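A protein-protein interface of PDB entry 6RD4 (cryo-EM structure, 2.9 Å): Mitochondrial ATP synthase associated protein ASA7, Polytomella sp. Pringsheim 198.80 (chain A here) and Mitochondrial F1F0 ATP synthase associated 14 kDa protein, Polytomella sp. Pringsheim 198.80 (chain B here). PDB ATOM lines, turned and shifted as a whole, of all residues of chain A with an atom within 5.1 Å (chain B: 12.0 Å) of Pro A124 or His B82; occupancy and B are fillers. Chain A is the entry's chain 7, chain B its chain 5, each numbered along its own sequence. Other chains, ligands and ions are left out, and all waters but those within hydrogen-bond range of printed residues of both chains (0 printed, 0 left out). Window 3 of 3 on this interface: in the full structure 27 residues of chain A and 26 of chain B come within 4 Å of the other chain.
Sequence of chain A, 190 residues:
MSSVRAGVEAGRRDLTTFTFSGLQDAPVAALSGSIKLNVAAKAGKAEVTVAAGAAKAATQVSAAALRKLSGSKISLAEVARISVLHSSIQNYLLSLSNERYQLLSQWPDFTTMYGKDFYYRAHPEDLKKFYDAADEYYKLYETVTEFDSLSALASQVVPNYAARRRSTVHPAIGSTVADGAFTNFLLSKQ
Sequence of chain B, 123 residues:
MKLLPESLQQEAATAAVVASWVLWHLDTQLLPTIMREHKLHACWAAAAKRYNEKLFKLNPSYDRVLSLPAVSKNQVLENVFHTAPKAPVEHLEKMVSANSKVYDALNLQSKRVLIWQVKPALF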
ATOM      1  N   TYR A 119      -3.810  21.086 -17.797  1.00  0.00           N
ATOM      2  CA  TYR A 119      -3.828  21.052 -19.251  1.00  0.00           C
ATOM      3  C   TYR A 119      -2.482  21.454 -19.810  1.00  0.00           C
ATOM      4  O   TYR A 119      -1.987  20.850 -20.762  1.00  0.00           O
ATOM      5  CB  TYR A 119      -4.918  21.984 -19.775  1.00  0.00           C
ATOM      6  CG  TYR A 119      -5.218  21.928 -21.251  1.00  0.00           C
ATOM      7  CD1 TYR A 119      -4.424  22.576 -22.168  1.00  0.00           C
ATOM      8  CD2 TYR A 119      -6.334  21.289 -21.718  1.00  0.00           C
ATOM      9  CE1 TYR A 119      -4.692  22.543 -23.484  1.00  0.00           C
ATOM     10  CE2 TYR A 119      -6.607  21.244 -23.050  1.00  0.00           C
ATOM     11  CZ  TYR A 119      -5.779  21.883 -23.919  1.00  0.00           C
ATOM     12  OH  TYR A 119      -6.033  21.875 -25.248  1.00  0.00           O
ATOM     13  N   ALA A 122       0.984  19.421 -18.832  1.00  0.00           N
ATOM     14  CA  ALA A 122       1.054  18.033 -19.240  1.00  0.00           C
ATOM     15  C   ALA A 122       1.441  17.908 -20.694  1.00  0.00           C
ATOM     16  O   ALA A 122       1.158  18.785 -21.506  1.00  0.00           O
ATOM     17  CB  ALA A 122      -0.279  17.337 -19.027  1.00  0.00           C
ATOM     18  N   HIS A 123       2.091  16.797 -20.993  1.00  0.00           N
ATOM     19  CA  HIS A 123       2.457  16.425 -22.344  1.00  0.00           C
ATOM     20  C   HIS A 123       1.205  16.350 -23.201  1.00  0.00           C
ATOM     21  O   HIS A 123       0.179  15.862 -22.735  1.00  0.00           O
ATOM     22  CB  HIS A 123       3.150  15.072 -22.295  1.00  0.00           C
ATOM     23  CG  HIS A 123       3.808  14.652 -23.560  1.00  0.00           C
ATOM     24  ND1 HIS A 123       5.156  14.410 -23.639  1.00  0.00           N
ATOM     25  CD2 HIS A 123       3.301  14.339 -24.770  1.00  0.00           C
ATOM     26  CE1 HIS A 123       5.456  14.010 -24.858  1.00  0.00           C
ATOM     27  NE2 HIS A 123       4.346  13.966 -25.567  1.00  0.00           N
ATOM     28  N   PRO A 124       1.240  16.858 -24.428  1.00  0.00           N
ATOM     29  CA  PRO A 124       0.024  16.883 -25.250  1.00  0.00           C
ATOM     30  C   PRO A 124      -0.521  15.524 -25.625  1.00  0.00           C
ATOM     31  O   PRO A 124      -1.676  15.434 -26.033  1.00  0.00           O
ATOM     32  CB  PRO A 124       0.479  17.651 -26.489  1.00  0.00           C
ATOM     33  CG  PRO A 124       1.563  18.475 -26.009  1.00  0.00           C
ATOM     34  CD  PRO A 124       2.288  17.707 -24.996  1.00  0.00           C
ATOM     35  N   GLU A 125       0.271  14.468 -25.519  1.00  0.00           N
ATOM     36  CA  GLU A 125      -0.215  13.127 -25.786  1.00  0.00           C
ATOM     37  C   GLU A 125      -0.673  12.417 -24.528  1.00  0.00           C
ATOM     38  O   GLU A 125      -1.497  11.511 -24.607  1.00  0.00           O
ATOM     39  CB  GLU A 125       0.861  12.312 -26.478  1.00  0.00           C
ATOM     40  CG  GLU A 125       1.193  12.836 -27.841  1.00  0.00           C
ATOM     41  CD  GLU A 125       0.036  12.705 -28.810  1.00  0.00           C
ATOM     42  OE1 GLU A 125      -0.729  11.726 -28.701  1.00  0.00           O
ATOM     43  OE2 GLU A 125      -0.110  13.582 -29.683  1.00  0.00           O
ATOM     44  N   ASP A 126      -0.128  12.781 -23.374  1.00  0.00           N
ATOM     45  CA  ASP A 126      -0.627  12.263 -22.115  1.00  0.00           C
ATOM     46  C   ASP A 126      -1.852  13.001 -21.646  1.00  0.00           C
ATOM     47  O   ASP A 126      -2.459  12.592 -20.663  1.00  0.00           O
ATOM     48  CB  ASP A 126       0.432  12.356 -21.035  1.00  0.00           C
ATOM     49  CG  ASP A 126       1.629  11.542 -21.351  1.00  0.00           C
ATOM     50  OD1 ASP A 126       1.545  10.712 -22.268  1.00  0.00           O
ATOM     51  OD2 ASP A 126       2.660  11.727 -20.682  1.00  0.00           O
ATOM     52  N   LEU A 127      -2.189  14.108 -22.274  1.00  0.00           N
ATOM     53  CA  LEU A 127      -3.454  14.747 -21.986  1.00  0.00           C
ATOM     54  C   LEU A 127      -4.551  14.205 -22.875  1.00  0.00           C
ATOM     55  O   LEU A 127      -5.700  14.110 -22.450  1.00  0.00           O
ATOM     56  CB  LEU A 127      -3.337  16.242 -22.181  1.00  0.00           C
ATOM     57  CG  LEU A 127      -4.529  16.991 -21.657  1.00  0.00           C
ATOM     58  CD1 LEU A 127      -4.414  17.164 -20.176  1.00  0.00           C
ATOM     59  CD2 LEU A 127      -4.652  18.245 -22.380  1.00  0.00           C
ATOM     60  N   LYS A 128      -4.232  13.843 -24.108  1.00  0.00           N
ATOM     61  CA  LYS A 128      -5.232  13.219 -24.955  1.00  0.00           C
ATOM     62  C   LYS A 128      -5.535  11.806 -24.503  1.00  0.00           C
ATOM     63  O   LYS A 128      -6.631  11.308 -24.752  1.00  0.00           O
ATOM     64  CB  LYS A 128      -4.776  13.208 -26.401  1.00  0.00           C
ATOM     65  CG  LYS A 128      -4.663  14.574 -26.989  1.00  0.00           C
ATOM     66  CD  LYS A 128      -4.518  14.506 -28.480  1.00  0.00           C
ATOM     67  CE  LYS A 128      -4.231  15.870 -29.037  1.00  0.00           C
ATOM     68  NZ  LYS A 128      -2.900  16.328 -28.586  1.00  0.00           N
ATOM     69  N   LYS B  73       1.693  32.049 -36.728  1.00  0.00           N
ATOM     70  CA  LYS B  73       0.687  32.284 -35.708  1.00  0.00           C
ATOM     71  C   LYS B  73      -0.301  31.140 -35.665  1.00  0.00           C
ATOM     72  O   LYS B  73      -0.850  30.836 -34.609  1.00  0.00           O
ATOM     73  CB  LYS B  73      -0.025  33.602 -35.972  1.00  0.00           C
ATOM     74  CG  LYS B  73      -0.964  34.043 -34.883  1.00  0.00           C
ATOM     75  CD  LYS B  73      -0.282  34.024 -33.538  1.00  0.00           C
ATOM     76  CE  LYS B  73      -1.183  34.553 -32.456  1.00  0.00           C
ATOM     77  NZ  LYS B  73      -0.380  34.838 -31.253  1.00  0.00           N
ATOM     78  N   ASN B  74      -0.533  30.503 -36.804  1.00  0.00           N
ATOM     79  CA  ASN B  74      -1.335  29.294 -36.847  1.00  0.00           C
ATOM     80  C   ASN B  74      -0.705  28.174 -36.047  1.00  0.00           C
ATOM     81  O   ASN B  74      -1.388  27.508 -35.271  1.00  0.00           O
ATOM     82  CB  ASN B  74      -1.497  28.840 -38.276  1.00  0.00           C
ATOM     83  CG  ASN B  74      -2.311  27.627 -38.376  1.00  0.00           C
ATOM     84  OD1 ASN B  74      -3.243  27.441 -37.619  1.00  0.00           O
ATOM     85  ND2 ASN B  74      -1.910  26.727 -39.242  1.00  0.00           N
ATOM     86  N   GLN B  75       0.590  27.940 -36.219  1.00  0.00           N
ATOM     87  CA  GLN B  75       1.246  26.842 -35.534  1.00  0.00           C
ATOM     88  C   GLN B  75       1.423  27.098 -34.054  1.00  0.00           C
ATOM     89  O   GLN B  75       1.744  26.168 -33.320  1.00  0.00           O
ATOM     90  CB  GLN B  75       2.604  26.583 -36.144  1.00  0.00           C
ATOM     91  CG  GLN B  75       2.544  26.250 -37.592  1.00  0.00           C
ATOM     92  CD  GLN B  75       3.849  25.740 -38.099  1.00  0.00           C
ATOM     93  OE1 GLN B  75       4.859  25.828 -37.424  1.00  0.00           O
ATOM     94  NE2 GLN B  75       3.835  25.173 -39.283  1.00  0.00           N
ATOM     95  N   VAL B  76       1.278  28.334 -33.604  1.00  0.00           N
ATOM     96  CA  VAL B  76       1.202  28.577 -32.176  1.00  0.00           C
ATOM     97  C   VAL B  76      -0.167  28.195 -31.665  1.00  0.00           C
ATOM     98  O   VAL B  76      -0.293  27.474 -30.676  1.00  0.00           O
ATOM     99  CB  VAL B  76       1.535  30.043 -31.877  1.00  0.00           C
ATOM    100  CG1 VAL B  76       1.329  30.345 -30.443  1.00  0.00           C
ATOM    101  CG2 VAL B  76       2.930  30.280 -32.204  1.00  0.00           C
ATOM    102  N   LEU B  77      -1.211  28.624 -32.363  1.00  0.00           N
ATOM    103  CA  LEU B  77      -2.574  28.385 -31.925  1.00  0.00           C
ATOM    104  C   LEU B  77      -2.997  26.940 -32.050  1.00  0.00           C
ATOM    105  O   LEU B  77      -4.055  26.581 -31.538  1.00  0.00           O
ATOM    106  CB  LEU B  77      -3.538  29.231 -32.730  1.00  0.00           C
ATOM    107  CG  LEU B  77      -3.549  30.718 -32.477  1.00  0.00           C
ATOM    108  CD1 LEU B  77      -4.737  31.272 -33.179  1.00  0.00           C
ATOM    109  CD2 LEU B  77      -3.624  30.993 -31.017  1.00  0.00           C
ATOM    110  N   GLU B  78      -2.245  26.112 -32.749  1.00  0.00           N
ATOM    111  CA  GLU B  78      -2.557  24.700 -32.774  1.00  0.00           C
ATOM    112  C   GLU B  78      -1.646  23.881 -31.886  1.00  0.00           C
ATOM    113  O   GLU B  78      -1.899  22.691 -31.709  1.00  0.00           O
ATOM    114  CB  GLU B  78      -2.499  24.173 -34.197  1.00  0.00           C
ATOM    115  CG  GLU B  78      -1.133  23.927 -34.711  1.00  0.00           C
ATOM    116  CD  GLU B  78      -1.164  23.527 -36.156  1.00  0.00           C
ATOM    117  OE1 GLU B  78      -2.270  23.516 -36.737  1.00  0.00           O
ATOM    118  OE2 GLU B  78      -0.087  23.236 -36.717  1.00  0.00           O
ATOM    119  N   ASN B  79      -0.605  24.474 -31.330  1.00  0.00           N
ATOM    120  CA  ASN B  79       0.241  23.814 -30.357  1.00  0.00           C
ATOM    121  C   ASN B  79      -0.063  24.259 -28.947  1.00  0.00           C
ATOM    122  O   ASN B  79       0.325  23.577 -28.000  1.00  0.00           O
ATOM    123  CB  ASN B  79       1.717  24.084 -30.640  1.00  0.00           C
ATOM    124  CG  ASN B  79       2.267  23.238 -31.741  1.00  0.00           C
ATOM    125  OD1 ASN B  79       3.088  22.366 -31.510  1.00  0.00           O
ATOM    126  ND2 ASN B  79       1.822  23.491 -32.950  1.00  0.00           N
ATOM    127  N   VAL B  80      -0.713  25.399 -28.786  1.00  0.00           N
ATOM    128  CA  VAL B  80      -1.131  25.867 -27.478  1.00  0.00           C
ATOM    129  C   VAL B  80      -2.547  25.403 -27.174  1.00  0.00           C
ATOM    130  O   VAL B  80      -2.845  25.005 -26.047  1.00  0.00           O
ATOM    131  CB  VAL B  80      -0.988  27.397 -27.450  1.00  0.00           C
ATOM    132  CG1 VAL B  80      -1.832  28.035 -26.402  1.00  0.00           C
ATOM    133  CG2 VAL B  80       0.444  27.758 -27.238  1.00  0.00           C
ATOM    134  N   PHE B  81      -3.394  25.339 -28.183  1.00  0.00           N
ATOM    135  CA  PHE B  81      -4.779  24.942 -28.044  1.00  0.00           C
ATOM    136  C   PHE B  81      -4.979  23.606 -28.722  1.00  0.00           C
ATOM    137  O   PHE B  81      -5.820  23.483 -29.611  1.00  0.00           O
ATOM    138  CB  PHE B  81      -5.691  25.989 -28.650  1.00  0.00           C
ATOM    139  CG  PHE B  81      -5.592  27.315 -27.995  1.00  0.00           C
ATOM    140  CD1 PHE B  81      -5.510  27.413 -26.625  1.00  0.00           C
ATOM    141  CD2 PHE B  81      -5.594  28.465 -28.742  1.00  0.00           C
ATOM    142  CE1 PHE B  81      -5.422  28.627 -26.016  1.00  0.00           C
ATOM    143  CE2 PHE B  81      -5.504  29.680 -28.135  1.00  0.00           C
ATOM    144  CZ  PHE B  81      -5.419  29.756 -26.772  1.00  0.00           C
ATOM    145  N   HIS B  82      -4.157  22.625 -28.356  1.00  0.00           N
ATOM    146  CA  HIS B  82      -4.096  21.373 -29.095  1.00  0.00           C
ATOM    147  C   HIS B  82      -5.355  20.532 -28.931  1.00  0.00           C
ATOM    148  O   HIS B  82      -5.826  19.930 -29.901  1.00  0.00           O
ATOM    149  CB  HIS B  82      -2.864  20.587 -28.671  1.00  0.00           C
ATOM    150  CG  HIS B  82      -2.650  20.527 -27.195  1.00  0.00           C
ATOM    151  ND1 HIS B  82      -3.120  19.497 -26.416  1.00  0.00           N
ATOM    152  CD2 HIS B  82      -1.985  21.352 -26.358  1.00  0.00           C
ATOM    153  CE1 HIS B  82      -2.763  19.695 -25.162  1.00  0.00           C
ATOM    154  NE2 HIS B  82      -2.074  20.816 -25.099  1.00  0.00           N
ATOM    155  N   THR B  83      -5.913  20.464 -27.730  1.00  0.00           N
ATOM    156  CA  THR B  83      -7.063  19.618 -27.440  1.00  0.00           C
ATOM    157  C   THR B  83      -8.212  20.500 -26.991  1.00  0.00           C
ATOM    158  O   THR B  83      -8.001  21.454 -26.245  1.00  0.00           O
ATOM    159  CB  THR B  83      -6.731  18.595 -26.341  1.00  0.00           C
ATOM    160  OG1 THR B  83      -5.471  17.986 -26.622  1.00  0.00           O
ATOM    161  CG2 THR B  83      -7.757  17.501 -26.278  1.00  0.00           C
ATOM    162  N   ALA B  84      -9.410  20.200 -27.453  1.00  0.00           N
ATOM    163  CA  ALA B  84     -10.588  20.915 -26.983  1.00  0.00           C
ATOM    164  C   ALA B  84     -10.837  20.570 -25.528  1.00  0.00           C
ATOM    165  O   ALA B  84     -11.039  19.394 -25.215  1.00  0.00           O
ATOM    166  CB  ALA B  84     -11.797  20.548 -27.818  1.00  0.00           C
ATOM    167  N   PRO B  85     -10.845  21.535 -24.620  1.00  0.00           N
ATOM    168  CA  PRO B  85     -10.847  21.216 -23.194  1.00  0.00           C
ATOM    169  C   PRO B  85     -12.197  20.704 -22.720  1.00  0.00           C
ATOM    170  O   PRO B  85     -13.244  20.982 -23.301  1.00  0.00           O
ATOM    171  CB  PRO B  85     -10.506  22.556 -22.543  1.00  0.00           C
ATOM    172  CG  PRO B  85     -11.058  23.538 -23.465  1.00  0.00           C
ATOM    173  CD  PRO B  85     -10.902  22.982 -24.849  1.00  0.00           C
ATOM    174  N   LYS B  86     -12.148  19.920 -21.648  1.00  0.00           N
ATOM    175  CA  LYS B  86     -13.346  19.295 -21.115  1.00  0.00           C
ATOM    176  C   LYS B  86     -14.164  20.317 -20.351  1.00  0.00           C
ATOM    177  O   LYS B  86     -13.642  21.014 -19.481  1.00  0.00           O
ATOM    178  CB  LYS B  86     -12.983  18.137 -20.205  1.00  0.00           C
ATOM    179  CG  LYS B  86     -12.453  16.933 -20.911  1.00  0.00           C
ATOM    180  CD  LYS B  86     -13.547  16.092 -21.483  1.00  0.00           C
ATOM    181  CE  LYS B  86     -13.024  14.709 -21.731  1.00  0.00           C
ATOM    182  NZ  LYS B  86     -13.994  13.893 -22.473  1.00  0.00           N
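The backbone NH (N) of Thr B83 is in hydrogen-bond range of the side-chain hydroxyl (OH) of Tyr A119.
O of Pro A124 is in hydrogen-bond range of NZ of Lys A128 (3.0 Å). ND1 of His B82 is in hydrogen-bond range of OG1 of Thr B83.
Tyr A119 touches His B82. Pro A124 touches His B82 (CA to CE1, 3.96 Å). Leu A127 touches His B82 (CD2 to CE1, 3.7 Å). ND1 of His B82 touches NZ of Lys A128, 3.8 Å away. Lys A128 touches Thr B83 (CE to OG1, 3.4 Å).
Pro A124 touches just one residue of chain B: His B82. His B82 touches just these residues of chain A: Tyr A119, Pro A124, Leu A127 and Lys A128. No residue of chain B comes within 4 Å of Ala A122. No residue of chain B comes within 4 Å of His A123. No residue of chain B comes within 4 Å of Glu A125. No residue of chain B comes within 4 Å of Asp A126. Leu A127 touches just one residue of chain B: His B82 (3.7 Å). Of the printed residues of chain A, Thr B83 touches Tyr A119 and Lys A128. Printed residues of chain B within 4 Å of Tyr A119: His B82 (3.5 Å) and Thr B83 (2.2 Å). Asn B74 touches none of the printed residues of chain A. Val B76 touches none of the printed residues of chain A. The nearest residue of chain B that does not touch Pro A124 is Thr B83 (4.6 Å).
Hydrophobic or aromatic side chains of chain B that line the printed part of chain A: His B82. Of the 8 printed residues of chain A, 4 touch a printed residue of chain B. Hydrophobic or aromatic side chains of chain A within 4 Å of the printed part of chain B: Tyr A119 and Leu A127. Along chain A the printed residues that touch a printed residue of chain B span positions 119 to 128. Among the printed residues, 6 pairs touch across the chains. Among the printed residues, no Asp or Glu carboxylate lies within 4 Å of a Lys or Arg side-chain nitrogen of the other chain.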
